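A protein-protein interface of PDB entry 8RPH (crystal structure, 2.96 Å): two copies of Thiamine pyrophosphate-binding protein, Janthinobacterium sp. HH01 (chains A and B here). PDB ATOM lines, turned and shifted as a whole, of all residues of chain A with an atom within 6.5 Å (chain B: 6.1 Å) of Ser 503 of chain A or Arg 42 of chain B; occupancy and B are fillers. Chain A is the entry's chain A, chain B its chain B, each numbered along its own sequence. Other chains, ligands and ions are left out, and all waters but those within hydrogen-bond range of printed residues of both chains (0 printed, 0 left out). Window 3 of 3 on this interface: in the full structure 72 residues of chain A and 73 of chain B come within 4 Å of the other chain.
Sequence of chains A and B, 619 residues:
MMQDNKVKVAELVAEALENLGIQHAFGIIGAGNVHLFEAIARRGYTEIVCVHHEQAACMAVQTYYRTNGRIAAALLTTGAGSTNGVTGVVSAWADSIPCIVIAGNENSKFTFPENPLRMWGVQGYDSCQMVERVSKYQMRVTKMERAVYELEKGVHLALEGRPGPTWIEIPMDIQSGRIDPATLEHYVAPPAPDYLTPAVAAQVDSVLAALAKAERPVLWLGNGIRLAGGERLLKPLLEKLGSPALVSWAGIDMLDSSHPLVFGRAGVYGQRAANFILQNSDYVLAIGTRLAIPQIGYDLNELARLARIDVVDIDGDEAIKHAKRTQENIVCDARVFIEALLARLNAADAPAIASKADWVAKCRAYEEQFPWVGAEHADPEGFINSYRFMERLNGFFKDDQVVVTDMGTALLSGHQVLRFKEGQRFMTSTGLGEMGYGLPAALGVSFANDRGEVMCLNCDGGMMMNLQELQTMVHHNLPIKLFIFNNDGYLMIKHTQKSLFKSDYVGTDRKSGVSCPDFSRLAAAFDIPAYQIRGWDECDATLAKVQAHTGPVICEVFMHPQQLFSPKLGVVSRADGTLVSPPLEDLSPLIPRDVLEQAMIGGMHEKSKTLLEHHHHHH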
ATOM      1  N   GLN A 497     -13.787  -3.667  -2.830  1.00  0.00           N
ATOM      2  CA  GLN A 497     -14.481  -2.735  -1.949  1.00  0.00           C
ATOM      3  C   GLN A 497     -15.922  -2.485  -2.380  1.00  0.00           C
ATOM      4  O   GLN A 497     -16.725  -2.027  -1.561  1.00  0.00           O
ATOM      5  CB  GLN A 497     -13.714  -1.411  -1.871  1.00  0.00           C
ATOM      6  CG  GLN A 497     -13.542  -0.692  -3.203  1.00  0.00           C
ATOM      7  CD  GLN A 497     -12.715   0.590  -3.104  1.00  0.00           C
ATOM      8  OE1 GLN A 497     -12.716   1.401  -4.027  1.00  0.00           O
ATOM      9  NE2 GLN A 497     -12.007   0.772  -1.995  1.00  0.00           N
ATOM     10  N   LYS A 498     -16.272  -2.771  -3.635  1.00  0.00           N
ATOM     11  CA  LYS A 498     -17.669  -2.660  -4.039  1.00  0.00           C
ATOM     12  C   LYS A 498     -18.487  -3.841  -3.536  1.00  0.00           C
ATOM     13  O   LYS A 498     -19.681  -3.688  -3.257  1.00  0.00           O
ATOM     14  CB  LYS A 498     -17.787  -2.555  -5.562  1.00  0.00           C
ATOM     15  CG  LYS A 498     -19.017  -1.787  -6.048  1.00  0.00           C
ATOM     16  CD  LYS A 498     -18.899  -0.292  -5.757  1.00  0.00           C
ATOM     17  CE  LYS A 498     -20.055   0.503  -6.355  1.00  0.00           C
ATOM     18  NZ  LYS A 498     -19.904   1.972  -6.134  1.00  0.00           N
ATOM     19  N   PHE A 501     -18.727  -3.027   0.618  1.00  0.00           N
ATOM     20  CA  PHE A 501     -19.333  -1.802   1.123  1.00  0.00           C
ATOM     21  C   PHE A 501     -20.408  -1.218   0.223  1.00  0.00           C
ATOM     22  O   PHE A 501     -21.282  -0.507   0.723  1.00  0.00           O
ATOM     23  CB  PHE A 501     -18.253  -0.736   1.351  1.00  0.00           C
ATOM     24  CG  PHE A 501     -17.033  -1.257   2.043  1.00  0.00           C
ATOM     25  CD1 PHE A 501     -17.105  -1.704   3.350  1.00  0.00           C
ATOM     26  CD2 PHE A 501     -15.813  -1.307   1.387  1.00  0.00           C
ATOM     27  CE1 PHE A 501     -15.986  -2.190   3.990  1.00  0.00           C
ATOM     28  CE2 PHE A 501     -14.689  -1.792   2.025  1.00  0.00           C
ATOM     29  CZ  PHE A 501     -14.776  -2.234   3.329  1.00  0.00           C
ATOM     30  N   LYS A 502     -20.371  -1.485  -1.080  1.00  0.00           N
ATOM     31  CA  LYS A 502     -21.380  -0.975  -2.004  1.00  0.00           C
ATOM     32  C   LYS A 502     -21.562   0.531  -1.829  1.00  0.00           C
ATOM     33  O   LYS A 502     -22.669   1.031  -1.610  1.00  0.00           O
ATOM     34  CB  LYS A 502     -22.707  -1.712  -1.813  1.00  0.00           C
ATOM     35  CG  LYS A 502     -22.682  -3.161  -2.267  1.00  0.00           C
ATOM     36  CD  LYS A 502     -23.977  -3.875  -1.909  1.00  0.00           C
ATOM     37  CE  LYS A 502     -24.117  -5.193  -2.656  1.00  0.00           C
ATOM     38  NZ  LYS A 502     -22.942  -6.089  -2.463  1.00  0.00           N
ATOM     39  N   SER A 503     -20.455   1.259  -1.915  1.00  0.00           N
ATOM     40  CA  SER A 503     -20.470   2.712  -1.787  1.00  0.00           C
ATOM     41  C   SER A 503     -19.447   3.277  -2.769  1.00  0.00           C
ATOM     42  O   SER A 503     -19.079   2.634  -3.759  1.00  0.00           O
ATOM     43  CB  SER A 503     -20.205   3.125  -0.332  1.00  0.00           C
ATOM     44  OG  SER A 503     -18.944   2.656   0.105  1.00  0.00           O
ATOM     45  N   ASP A 504     -18.981   4.496  -2.505  1.00  0.00           N
ATOM     46  CA  ASP A 504     -18.030   5.142  -3.395  1.00  0.00           C
ATOM     47  C   ASP A 504     -16.645   4.521  -3.250  1.00  0.00           C
ATOM     48  O   ASP A 504     -16.261   4.042  -2.180  1.00  0.00           O
ATOM     49  CB  ASP A 504     -17.957   6.641  -3.104  1.00  0.00           C
ATOM     50  CG  ASP A 504     -19.196   7.383  -3.561  1.00  0.00           C
ATOM     51  OD1 ASP A 504     -19.774   6.994  -4.598  1.00  0.00           O
ATOM     52  OD2 ASP A 504     -19.589   8.357  -2.887  1.00  0.00           O
ATOM     53  N   TYR A 505     -15.893   4.538  -4.345  1.00  0.00           N
ATOM     54  CA  TYR A 505     -14.549   3.983  -4.336  1.00  0.00           C
ATOM     55  C   TYR A 505     -13.641   4.787  -3.413  1.00  0.00           C
ATOM     56  O   TYR A 505     -13.866   5.974  -3.155  1.00  0.00           O
ATOM     57  CB  TYR A 505     -13.974   3.956  -5.754  1.00  0.00           C
ATOM     58  CG  TYR A 505     -14.652   2.962  -6.677  1.00  0.00           C
ATOM     59  CD1 TYR A 505     -14.992   1.689  -6.233  1.00  0.00           C
ATOM     60  CD2 TYR A 505     -14.959   3.298  -7.990  1.00  0.00           C
ATOM     61  CE1 TYR A 505     -15.613   0.779  -7.071  1.00  0.00           C
ATOM     62  CE2 TYR A 505     -15.582   2.393  -8.836  1.00  0.00           C
ATOM     63  CZ  TYR A 505     -15.904   1.136  -8.371  1.00  0.00           C
ATOM     64  OH  TYR A 505     -16.524   0.236  -9.208  1.00  0.00           O
ATOM     65  N   VAL A 506     -12.608   4.118  -2.901  1.00  0.00           N
ATOM     66  CA  VAL A 506     -11.658   4.717  -1.968  1.00  0.00           C
ATOM     67  C   VAL A 506     -10.259   4.268  -2.368  1.00  0.00           C
ATOM     68  O   VAL A 506      -9.962   3.068  -2.361  1.00  0.00           O
ATOM     69  CB  VAL A 506     -11.957   4.328  -0.508  1.00  0.00           C
ATOM     70  CG1 VAL A 506     -10.917   4.920   0.431  1.00  0.00           C
ATOM     71  CG2 VAL A 506     -13.352   4.794  -0.109  1.00  0.00           C
ATOM     72  N   PHE B  37      -8.800   1.301   4.946  1.00  0.00           N
ATOM     73  CA  PHE B  37      -9.016   2.391   3.999  1.00  0.00           C
ATOM     74  C   PHE B  37     -10.448   2.903   4.074  1.00  0.00           C
ATOM     75  O   PHE B  37     -10.689   4.115   4.111  1.00  0.00           O
ATOM     76  CB  PHE B  37      -8.693   1.920   2.580  1.00  0.00           C
ATOM     77  CG  PHE B  37      -7.287   2.214   2.148  1.00  0.00           C
ATOM     78  CD1 PHE B  37      -6.224   1.488   2.655  1.00  0.00           C
ATOM     79  CD2 PHE B  37      -7.029   3.216   1.224  1.00  0.00           C
ATOM     80  CE1 PHE B  37      -4.929   1.758   2.256  1.00  0.00           C
ATOM     81  CE2 PHE B  37      -5.738   3.487   0.819  1.00  0.00           C
ATOM     82  CZ  PHE B  37      -4.688   2.759   1.337  1.00  0.00           C
ATOM     83  N   GLU B  38     -11.417   1.986   4.096  1.00  0.00           N
ATOM     84  CA  GLU B  38     -12.816   2.393   4.151  1.00  0.00           C
ATOM     85  C   GLU B  38     -13.104   3.162   5.435  1.00  0.00           C
ATOM     86  O   GLU B  38     -13.658   4.265   5.402  1.00  0.00           O
ATOM     87  CB  GLU B  38     -13.721   1.166   4.044  1.00  0.00           C
ATOM     88  CG  GLU B  38     -15.184   1.487   3.785  1.00  0.00           C
ATOM     89  CD  GLU B  38     -15.431   2.005   2.379  1.00  0.00           C
ATOM     90  OE1 GLU B  38     -14.484   1.994   1.561  1.00  0.00           O
ATOM     91  OE2 GLU B  38     -16.571   2.422   2.091  1.00  0.00           O
ATOM     92  N   ALA B  39     -12.709   2.597   6.579  1.00  0.00           N
ATOM     93  CA  ALA B  39     -13.030   3.214   7.860  1.00  0.00           C
ATOM     94  C   ALA B  39     -12.353   4.569   8.015  1.00  0.00           C
ATOM     95  O   ALA B  39     -12.967   5.524   8.502  1.00  0.00           O
ATOM     96  CB  ALA B  39     -12.629   2.280   9.002  1.00  0.00           C
ATOM     97  N   ILE B  40     -11.086   4.677   7.608  1.00  0.00           N
ATOM     98  CA  ILE B  40     -10.384   5.952   7.726  1.00  0.00           C
ATOM     99  C   ILE B  40     -11.024   6.999   6.824  1.00  0.00           C
ATOM    100  O   ILE B  40     -11.183   8.162   7.214  1.00  0.00           O
ATOM    101  CB  ILE B  40      -8.889   5.772   7.404  1.00  0.00           C
ATOM    102  CG1 ILE B  40      -8.238   4.854   8.440  1.00  0.00           C
ATOM    103  CG2 ILE B  40      -8.183   7.129   7.358  1.00  0.00           C
ATOM    104  CD1 ILE B  40      -6.802   4.506   8.130  1.00  0.00           C
ATOM    105  N   ALA B  41     -11.385   6.608   5.601  1.00  0.00           N
ATOM    106  CA  ALA B  41     -11.995   7.553   4.674  1.00  0.00           C
ATOM    107  C   ALA B  41     -13.339   8.044   5.199  1.00  0.00           C
ATOM    108  O   ALA B  41     -13.580   9.253   5.283  1.00  0.00           O
ATOM    109  CB  ALA B  41     -12.156   6.901   3.301  1.00  0.00           C
ATOM    110  N   ARG B  42     -14.225   7.116   5.569  1.00  0.00           N
ATOM    111  CA  ARG B  42     -15.568   7.499   5.991  1.00  0.00           C
ATOM    112  C   ARG B  42     -15.563   8.364   7.243  1.00  0.00           C
ATOM    113  O   ARG B  42     -16.539   9.080   7.489  1.00  0.00           O
ATOM    114  CB  ARG B  42     -16.426   6.251   6.224  1.00  0.00           C
ATOM    115  CG  ARG B  42     -16.618   5.364   4.988  1.00  0.00           C
ATOM    116  CD  ARG B  42     -16.866   6.185   3.723  1.00  0.00           C
ATOM    117  NE  ARG B  42     -16.974   5.364   2.522  1.00  0.00           N
ATOM    118  CZ  ARG B  42     -16.985   5.849   1.287  1.00  0.00           C
ATOM    119  NH1 ARG B  42     -16.891   7.150   1.053  1.00  0.00           N
ATOM    120  NH2 ARG B  42     -17.089   5.009   0.261  1.00  0.00           N
ATOM    121  N   ARG B  43     -14.494   8.321   8.038  1.00  0.00           N
ATOM    122  CA  ARG B  43     -14.419   9.200   9.199  1.00  0.00           C
ATOM    123  C   ARG B  43     -13.997  10.608   8.798  1.00  0.00           C
ATOM    124  O   ARG B  43     -14.465  11.590   9.384  1.00  0.00           O
ATOM    125  CB  ARG B  43     -13.454   8.625  10.233  1.00  0.00           C
ATOM    126  CG  ARG B  43     -13.462   9.386  11.540  1.00  0.00           C
ATOM    127  CD  ARG B  43     -12.693   8.657  12.620  1.00  0.00           C
ATOM    128  NE  ARG B  43     -12.830   9.325  13.909  1.00  0.00           N
ATOM    129  CZ  ARG B  43     -13.833   9.127  14.754  1.00  0.00           C
ATOM    130  NH1 ARG B  43     -14.801   8.263  14.491  1.00  0.00           N
ATOM    131  NH2 ARG B  43     -13.869   9.816  15.890  1.00  0.00           N
ATOM    132  N   GLY B  44     -13.117  10.724   7.807  1.00  0.00           N
ATOM    133  CA  GLY B  44     -12.746  12.007   7.252  1.00  0.00           C
ATOM    134  C   GLY B  44     -11.705  12.789   8.025  1.00  0.00           C
ATOM    135  O   GLY B  44     -11.348  13.893   7.597  1.00  0.00           O
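The side-chain hydroxyl (OG) of Ser 503 of chain A lies within hydrogen-bond range of the guanidinium group (NH2) of Arg 42 of chain B.
OG of Ser 503 of chain A sits at hydrogen-bond distance from OE2 of Glu 38 of chain B (3.1 Å).
NH2 of Arg 42 of chain B is in hydrogen-bond range of O of Asp 504 of chain A, 2.8 Å away.
The side-chain carboxylate (OE2) of Glu 38 of chain B lies within salt-bridge range of the guanidinium group (NE) of Arg 42 of chain B.
The side-chain amino group of Lys 498 of chain A lies within hydrogen-bond range of the backbone carbonyl oxygen of Ser 503 of chain A (2.6 Å).
The backbone NH (N) of Val 506 of chain A is in hydrogen-bond range of the side-chain amide oxygen (OE1) of Gln 497 of chain A (2.9 Å).
Among the printed residues, pairs that only touch across the chains: Val 506 of chain A with Glu 38 of chain B (3.5 Å), Phe 501 of chain A with Glu 38 of chain B (3.5 Å), Val 506 of chain A with Ala 41 of chain B (3.7 Å), Val 506 of chain A with Arg 42 of chain B (3.8 Å) and Val 506 of chain A with Phe 37 of chain B (3.8 Å).
Gln 497 of chain A touches none of the printed residues of chain B.
Of the printed residues of chain B, Val 506 of chain A touches Phe 37, Glu 38, Ala 41 and Arg 42.
Printed residues of chain A within 4 Å of Phe 37 of chain B: Val 506 (3.8 Å).
Printed residues of chain A within 4 Å of Glu 38 of chain B: Phe 501, Ser 503 and Val 506.
Ala 39 of chain B touches none of the printed residues of chain A.
Printed residues of chain A within 4 Å of Ala 41 of chain B: Val 506 (3.7 Å).
The nearest residue of chain A that does not touch Arg 42 of chain B is Tyr 505 of chain A (4.8 Å).
Hydrophobic or aromatic side chains of chain A within 4 Å of the printed part of chain B: Phe 501 and Val 506.
No position is printed for both chains.
Of the 8 pairs that touch across the chains among the printed residues, none has its exchanged pair printed and touching as well.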
